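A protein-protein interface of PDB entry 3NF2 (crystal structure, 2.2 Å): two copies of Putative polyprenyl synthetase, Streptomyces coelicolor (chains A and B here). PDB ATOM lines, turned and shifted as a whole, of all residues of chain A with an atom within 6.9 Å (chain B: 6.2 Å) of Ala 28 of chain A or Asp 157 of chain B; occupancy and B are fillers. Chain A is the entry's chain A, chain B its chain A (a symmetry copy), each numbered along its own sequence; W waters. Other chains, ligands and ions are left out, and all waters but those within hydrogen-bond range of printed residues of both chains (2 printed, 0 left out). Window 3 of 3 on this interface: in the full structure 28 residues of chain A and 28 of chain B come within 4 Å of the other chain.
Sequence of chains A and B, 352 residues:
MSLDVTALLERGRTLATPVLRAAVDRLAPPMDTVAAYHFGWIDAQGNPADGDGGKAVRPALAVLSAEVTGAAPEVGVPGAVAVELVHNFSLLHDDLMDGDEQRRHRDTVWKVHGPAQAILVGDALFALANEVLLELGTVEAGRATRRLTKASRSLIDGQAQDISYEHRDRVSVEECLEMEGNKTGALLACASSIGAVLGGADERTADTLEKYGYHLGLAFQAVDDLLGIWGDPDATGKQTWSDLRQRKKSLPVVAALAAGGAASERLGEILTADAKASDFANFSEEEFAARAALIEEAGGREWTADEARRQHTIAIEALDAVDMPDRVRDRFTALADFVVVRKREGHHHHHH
Among the printed residues, merely in contact across the chains: Met 31 of chain A with Asp 157 of chain B (3.6 Å), Leu 120 of chain A with Ile 156 of chain B (3.6 Å), Leu 120 of chain A with Gln 159 of chain B (3.7 Å), Met 31 of chain A with Ile 156 of chain B (3.7 Å), Ala 124 of chain A with Ile 156 of chain B (3.8 Å), Leu 120 of chain A with Ala 160 of chain B (3.8 Å), Ala 28 of chain A with Asp 157 of chain B (3.9 Å) and Met 31 of chain A with Ala 160 of chain B (3.99 Å).
Water W2 bridges OD2 of Asp 157 of chain B (2.7 Å) and N of Ala 28 of chain A (2.9 Å). Water W1 bridges the backbone carbonyl oxygen (O) of Ala 124 of chain A (2.8 Å) and the guanidinium group (NH1) of Arg 153 of chain B (3.0 Å).
No position is printed for both chains. Of the 8 pairs that touch across the chains among the printed residues, none has its exchanged pair printed and touching as well.
Hydrophobic or aromatic side chains of chain B that line the printed part of chain A: Ile 156 and Ala 160. Along chain B the printed residues that touch a printed residue of chain A span positions 156 to 160. Of the 12 printed residues of chain A, 4 touch a printed residue of chain B. Among the printed residues, no Asp or Glu carboxylate lies within 4 Å of a Lys or Arg side-chain nitrogen of the other chain.
Of chain B, only Asp 157 (3.9 Å) comes within 4 Å of Ala 28 of chain A. Printed residues of chain B within 4 Å of Met 31 of chain A: Ile 156 (3.7 Å), Asp 157 (3.6 Å) and Ala 160 (3.99 Å). Of the printed residues of chain B, Leu 120 of chain A touches Ile 156, Gln 159 and Ala 160. Of the printed residues of chain B, Ala 124 of chain A touches Ile 156. Of the printed residues of chain A, Ile 156 of chain B touches Met 31, Leu 120 and Ala 124. Asp 157 of chain B touches just these residues of chain A: Ala 28 and Met 31. Printed residues of chain A within 4 Å of Gln 159 of chain B: Leu 120. The nearest residue of chain B that does not touch Ala 28 of chain A is Ala 160 of chain B (4.8 Å).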
ATOM      1  N   VAL A  24       2.096 -18.338 -11.845  1.00  0.00           N
ATOM      2  CA  VAL A  24       0.910 -18.621 -11.033  1.00  0.00           C
ATOM      3  C   VAL A  24       0.287 -19.997 -11.345  1.00  0.00           C
ATOM      4  O   VAL A  24      -0.121 -20.735 -10.435  1.00  0.00           O
ATOM      5  CB  VAL A  24      -0.112 -17.468 -11.177  1.00  0.00           C
ATOM      6  CG1 VAL A  24      -1.554 -17.932 -10.930  1.00  0.00           C
ATOM      7  CG2 VAL A  24       0.283 -16.304 -10.264  1.00  0.00           C
ATOM      8  N   ASP A  25       0.247 -20.349 -12.628  1.00  0.00           N
ATOM      9  CA  ASP A  25      -0.245 -21.663 -13.062  1.00  0.00           C
ATOM     10  C   ASP A  25       0.602 -22.838 -12.523  1.00  0.00           C
ATOM     11  O   ASP A  25       0.123 -23.972 -12.444  1.00  0.00           O
ATOM     12  CB  ASP A  25      -0.354 -21.710 -14.601  1.00  0.00           C
ATOM     13  CG  ASP A  25      -1.477 -20.804 -15.154  1.00  0.00           C
ATOM     14  OD1 ASP A  25      -1.703 -20.819 -16.378  1.00  0.00           O
ATOM     15  OD2 ASP A  25      -2.139 -20.079 -14.380  1.00  0.00           O
ATOM     16  N   ARG A  26       1.847 -22.547 -12.141  1.00  0.00           N
ATOM     17  CA  ARG A  26       2.783 -23.545 -11.613  1.00  0.00           C
ATOM     18  C   ARG A  26       2.615 -23.849 -10.118  1.00  0.00           C
ATOM     19  O   ARG A  26       3.275 -24.737  -9.595  1.00  0.00           O
ATOM     20  CB  ARG A  26       4.218 -23.093 -11.874  1.00  0.00           C
ATOM     21  CG  ARG A  26       4.659 -23.202 -13.322  1.00  0.00           C
ATOM     22  CD  ARG A  26       5.551 -24.405 -13.546  1.00  0.00           C
ATOM     23  NE  ARG A  26       6.899 -24.178 -13.025  1.00  0.00           N
ATOM     24  CZ  ARG A  26       7.775 -25.142 -12.754  1.00  0.00           C
ATOM     25  NH1 ARG A  26       7.453 -26.417 -12.944  1.00  0.00           N
ATOM     26  NH2 ARG A  26       8.975 -24.830 -12.284  1.00  0.00           N
ATOM     27  N   LEU A  27       1.755 -23.105  -9.429  1.00  0.00           N
ATOM     28  CA  LEU A  27       1.486 -23.341  -8.006  1.00  0.00           C
ATOM     29  C   LEU A  27       0.731 -24.653  -7.779  1.00  0.00           C
ATOM     30  O   LEU A  27      -0.135 -25.032  -8.564  1.00  0.00           O
ATOM     31  CB  LEU A  27       0.667 -22.195  -7.407  1.00  0.00           C
ATOM     32  CG  LEU A  27       1.170 -20.757  -7.275  1.00  0.00           C
ATOM     33  CD1 LEU A  27      -0.024 -19.882  -6.895  1.00  0.00           C
ATOM     34  CD2 LEU A  27       2.266 -20.619  -6.236  1.00  0.00           C
ATOM     35  N   ALA A  28       1.054 -25.325  -6.684  1.00  0.00           N
ATOM     36  CA  ALA A  28       0.426 -26.593  -6.332  1.00  0.00           C
ATOM     37  C   ALA A  28      -1.094 -26.423  -6.128  1.00  0.00           C
ATOM     38  O   ALA A  28      -1.523 -25.447  -5.515  1.00  0.00           O
ATOM     39  CB  ALA A  28       1.085 -27.164  -5.080  1.00  0.00           C
ATOM     40  N   PRO A  29      -1.907 -27.346  -6.686  1.00  0.00           N
ATOM     41  CA  PRO A  29      -3.372 -27.354  -6.496  1.00  0.00           C
ATOM     42  C   PRO A  29      -3.800 -27.346  -5.020  1.00  0.00           C
ATOM     43  O   PRO A  29      -3.179 -28.031  -4.207  1.00  0.00           O
ATOM     44  CB  PRO A  29      -3.787 -28.665  -7.161  1.00  0.00           C
ATOM     45  CG  PRO A  29      -2.796 -28.808  -8.287  1.00  0.00           C
ATOM     46  CD  PRO A  29      -1.484 -28.328  -7.705  1.00  0.00           C
ATOM     47  N   PRO A  30      -4.852 -26.575  -4.662  1.00  0.00           N
ATOM     48  CA  PRO A  30      -5.750 -25.766  -5.497  1.00  0.00           C
ATOM     49  C   PRO A  30      -5.281 -24.324  -5.726  1.00  0.00           C
ATOM     50  O   PRO A  30      -6.024 -23.530  -6.312  1.00  0.00           O
ATOM     51  CB  PRO A  30      -7.028 -25.730  -4.662  1.00  0.00           C
ATOM     52  CG  PRO A  30      -6.524 -25.693  -3.247  1.00  0.00           C
ATOM     53  CD  PRO A  30      -5.221 -26.478  -3.233  1.00  0.00           C
ATOM     54  N   MET A  31      -4.067 -23.998  -5.279  1.00  0.00           N
ATOM     55  CA  MET A  31      -3.576 -22.612  -5.278  1.00  0.00           C
ATOM     56  C   MET A  31      -3.502 -21.977  -6.664  1.00  0.00           C
ATOM     57  O   MET A  31      -3.721 -20.783  -6.797  1.00  0.00           O
ATOM     58  CB  MET A  31      -2.226 -22.488  -4.558  1.00  0.00           C
ATOM     59  CG  MET A  31      -2.214 -23.075  -3.145  1.00  0.00           C
ATOM     60  SD  MET A  31      -0.780 -22.577  -2.180  1.00  0.00           S
ATOM     61  CE  MET A  31       0.473 -23.544  -2.994  1.00  0.00           C
ATOM     62  N   ASP A  32      -3.229 -22.776  -7.693  1.00  0.00           N
ATOM     63  CA  ASP A  32      -3.175 -22.260  -9.064  1.00  0.00           C
ATOM     64  C   ASP A  32      -4.547 -21.787  -9.564  1.00  0.00           C
ATOM     65  O   ASP A  32      -4.635 -20.742 -10.201  1.00  0.00           O
ATOM     66  CB  ASP A  32      -2.551 -23.281 -10.032  1.00  0.00           C
ATOM     67  CG  ASP A  32      -3.310 -24.599 -10.080  1.00  0.00           C
ATOM     68  OD1 ASP A  32      -3.981 -24.962  -9.091  1.00  0.00           O
ATOM     69  OD2 ASP A  32      -3.236 -25.282 -11.114  1.00  0.00           O
ATOM     70  N   THR A  33      -5.607 -22.538  -9.251  1.00  0.00           N
ATOM     71  CA  THR A  33      -6.956 -22.171  -9.685  1.00  0.00           C
ATOM     72  C   THR A  33      -7.535 -21.043  -8.844  1.00  0.00           C
ATOM     73  O   THR A  33      -8.195 -20.145  -9.368  1.00  0.00           O
ATOM     74  CB  THR A  33      -7.941 -23.383  -9.731  1.00  0.00           C
ATOM     75  OG1 THR A  33      -8.029 -24.012  -8.441  1.00  0.00           O
ATOM     76  CG2 THR A  33      -7.487 -24.406 -10.770  1.00  0.00           C
ATOM     77  N   LEU A 120      -3.763 -18.715   2.279  1.00  0.00           N
ATOM     78  CA  LEU A 120      -2.787 -19.630   1.705  1.00  0.00           C
ATOM     79  C   LEU A 120      -2.224 -19.106   0.385  1.00  0.00           C
ATOM     80  O   LEU A 120      -1.007 -18.976   0.224  1.00  0.00           O
ATOM     81  CB  LEU A 120      -3.462 -20.974   1.484  1.00  0.00           C
ATOM     82  CG  LEU A 120      -2.657 -22.156   0.963  1.00  0.00           C
ATOM     83  CD1 LEU A 120      -1.752 -22.711   2.050  1.00  0.00           C
ATOM     84  CD2 LEU A 120      -3.606 -23.226   0.418  1.00  0.00           C
ATOM     85  N   ALA A 124       1.428 -17.737  -0.719  1.00  0.00           N
ATOM     86  CA  ALA A 124       2.107 -18.378  -1.819  1.00  0.00           C
ATOM     87  C   ALA A 124       2.612 -17.346  -2.813  1.00  0.00           C
ATOM     88  O   ALA A 124       3.709 -17.487  -3.328  1.00  0.00           O
ATOM     89  CB  ALA A 124       1.186 -19.365  -2.500  1.00  0.00           C
ATOM     90  N   SER B 152      10.076 -21.977   2.540  1.00  0.00           N
ATOM     91  CA  SER B 152       8.829 -21.301   2.852  1.00  0.00           C
ATOM     92  C   SER B 152       7.776 -21.649   1.816  1.00  0.00           C
ATOM     93  O   SER B 152       6.627 -21.882   2.176  1.00  0.00           O
ATOM     94  CB  SER B 152       9.035 -19.791   2.938  1.00  0.00           C
ATOM     95  OG  SER B 152       9.356 -19.278   1.660  1.00  0.00           O
ATOM     96  N   ARG B 153       8.173 -21.714   0.543  1.00  0.00           N
ATOM     97  CA  ARG B 153       7.265 -22.129  -0.544  1.00  0.00           C
ATOM     98  C   ARG B 153       6.811 -23.559  -0.293  1.00  0.00           C
ATOM     99  O   ARG B 153       5.651 -23.923  -0.551  1.00  0.00           O
ATOM    100  CB  ARG B 153       7.928 -22.036  -1.928  1.00  0.00           C
ATOM    101  CG  ARG B 153       8.382 -20.627  -2.340  1.00  0.00           C
ATOM    102  CD  ARG B 153       8.109 -20.269  -3.804  1.00  0.00           C
ATOM    103  NE  ARG B 153       8.446 -21.338  -4.743  1.00  0.00           N
ATOM    104  CZ  ARG B 153       7.603 -21.856  -5.639  1.00  0.00           C
ATOM    105  NH1 ARG B 153       6.358 -21.402  -5.739  1.00  0.00           N
ATOM    106  NH2 ARG B 153       8.013 -22.826  -6.449  1.00  0.00           N
ATOM    107  N   SER B 154       7.734 -24.352   0.250  1.00  0.00           N
ATOM    108  CA  SER B 154       7.483 -25.741   0.586  1.00  0.00           C
ATOM    109  C   SER B 154       6.475 -25.920   1.710  1.00  0.00           C
ATOM    110  O   SER B 154       5.569 -26.723   1.577  1.00  0.00           O
ATOM    111  CB  SER B 154       8.791 -26.446   0.927  1.00  0.00           C
ATOM    112  OG  SER B 154       9.517 -26.721  -0.253  1.00  0.00           O
ATOM    113  N   LEU B 155       6.635 -25.180   2.804  1.00  0.00           N
ATOM    114  CA  LEU B 155       5.678 -25.184   3.919  1.00  0.00           C
ATOM    115  C   LEU B 155       4.270 -24.771   3.474  1.00  0.00           C
ATOM    116  O   LEU B 155       3.270 -25.303   3.969  1.00  0.00           O
ATOM    117  CB  LEU B 155       6.139 -24.198   4.996  1.00  0.00           C
ATOM    118  CG  LEU B 155       7.270 -24.583   5.951  1.00  0.00           C
ATOM    119  CD1 LEU B 155       7.867 -23.313   6.532  1.00  0.00           C
ATOM    120  CD2 LEU B 155       6.729 -25.468   7.071  1.00  0.00           C
ATOM    121  N   ILE B 156       4.202 -23.794   2.567  1.00  0.00           N
ATOM    122  CA  ILE B 156       2.932 -23.360   1.979  1.00  0.00           C
ATOM    123  C   ILE B 156       2.325 -24.515   1.169  1.00  0.00           C
ATOM    124  O   ILE B 156       1.127 -24.812   1.315  1.00  0.00           O
ATOM    125  CB  ILE B 156       3.107 -22.064   1.131  1.00  0.00           C
ATOM    126  CG1 ILE B 156       3.457 -20.876   2.033  1.00  0.00           C
ATOM    127  CG2 ILE B 156       1.854 -21.751   0.346  1.00  0.00           C
ATOM    128  CD1 ILE B 156       4.254 -19.789   1.323  1.00  0.00           C
ATOM    129  N   ASP B 157       3.168 -25.189   0.374  1.00  0.00           N
ATOM    130  CA  ASP B 157       2.773 -26.392  -0.384  1.00  0.00           C
ATOM    131  C   ASP B 157       2.221 -27.470   0.521  1.00  0.00           C
ATOM    132  O   ASP B 157       1.200 -28.081   0.203  1.00  0.00           O
ATOM    133  CB  ASP B 157       3.946 -26.995  -1.160  1.00  0.00           C
ATOM    134  CG  ASP B 157       4.316 -26.199  -2.398  1.00  0.00           C
ATOM    135  OD1 ASP B 157       5.363 -26.524  -3.007  1.00  0.00           O
ATOM    136  OD2 ASP B 157       3.577 -25.255  -2.753  1.00  0.00           O
ATOM    137  N   GLY B 158       2.896 -27.690   1.652  1.00  0.00           N
ATOM    138  CA  GLY B 158       2.508 -28.724   2.603  1.00  0.00           C
ATOM    139  C   GLY B 158       1.149 -28.454   3.200  1.00  0.00           C
ATOM    140  O   GLY B 158       0.340 -29.367   3.344  1.00  0.00           O
ATOM    141  N   GLN B 159       0.919 -27.190   3.534  1.00  0.00           N
ATOM    142  CA  GLN B 159      -0.379 -26.717   3.988  1.00  0.00           C
ATOM    143  C   GLN B 159      -1.478 -26.821   2.915  1.00  0.00           C
ATOM    144  O   GLN B 159      -2.613 -27.180   3.237  1.00  0.00           O
ATOM    145  CB  GLN B 159      -0.254 -25.287   4.536  1.00  0.00           C
ATOM    146  CG  GLN B 159      -1.528 -24.735   5.152  1.00  0.00           C
ATOM    147  CD  GLN B 159      -2.010 -25.528   6.355  1.00  0.00           C
ATOM    148  OE1 GLN B 159      -1.243 -26.270   6.976  1.00  0.00           O
ATOM    149  NE2 GLN B 159      -3.289 -25.365   6.694  1.00  0.00           N
ATOM    150  N   ALA B 160      -1.141 -26.535   1.655  1.00  0.00           N
ATOM    151  CA  ALA B 160      -2.071 -26.745   0.534  1.00  0.00           C
ATOM    152  C   ALA B 160      -2.463 -28.208   0.421  1.00  0.00           C
ATOM    153  O   ALA B 160      -3.641 -28.535   0.231  1.00  0.00           O
ATOM    154  CB  ALA B 160      -1.470 -26.260  -0.796  1.00  0.00           C
ATOM    155  N   GLN B 161      -1.468 -29.083   0.551  1.00  0.00           N
ATOM    156  CA  GLN B 161      -1.701 -30.519   0.577  1.00  0.00           C
ATOM    157  C   GLN B 161      -2.622 -30.896   1.741  1.00  0.00           C
ATOM    158  O   GLN B 161      -3.575 -31.657   1.560  1.00  0.00           O
ATOM    159  CB  GLN B 161      -0.364 -31.277   0.616  1.00  0.00           C
ATOM    160  CG  GLN B 161       0.338 -31.281  -0.745  1.00  0.00           C
ATOM    161  CD  GLN B 161       1.868 -31.422  -0.698  1.00  0.00           C
ATOM    162  OE1 GLN B 161       2.475 -31.635   0.357  1.00  0.00           O
ATOM    163  NE2 GLN B 161       2.494 -31.301  -1.869  1.00  0.00           N
ATOM    164  N   ASP B 162      -2.361 -30.333   2.916  1.00  0.00           N
ATOM    165  CA  ASP B 162      -3.188 -30.608   4.096  1.00  0.00           C
ATOM    166  C   ASP B 162      -4.657 -30.272   3.832  1.00  0.00           C
ATOM    167  O   ASP B 162      -5.524 -31.126   3.995  1.00  0.00           O
ATOM    168  CB  ASP B 162      -2.671 -29.856   5.320  1.00  0.00           C
ATOM    169  CG  ASP B 162      -3.308 -30.337   6.603  1.00  0.00           C
ATOM    170  OD1 ASP B 162      -2.638 -31.071   7.353  1.00  0.00           O
ATOM    171  OD2 ASP B 162      -4.484 -30.002   6.863  1.00  0.00           O
ATOM    172  N   ASN B 182       7.352 -31.570   3.067  1.00  0.00           N
ATOM    173  CA  ASN B 182       7.091 -30.164   2.947  1.00  0.00           C
ATOM    174  C   ASN B 182       6.906 -29.478   4.285  1.00  0.00           C
ATOM    175  O   ASN B 182       7.457 -28.451   4.532  1.00  0.00           O
ATOM    176  CB  ASN B 182       5.867 -29.930   2.080  1.00  0.00           C
ATOM    177  CG  ASN B 182       6.155 -30.026   0.619  1.00  0.00           C
ATOM    178  OD1 ASN B 182       7.231 -29.712   0.164  1.00  0.00           O
ATOM    179  ND2 ASN B 182       5.190 -30.455  -0.120  1.00  0.00           N
HETATM  180  O   HOH W   1       4.781 -20.011  -3.588  1.00  0.00           O
HETATM  181  O   HOH W   2       3.068 -23.917  -5.076  1.00  0.00           O
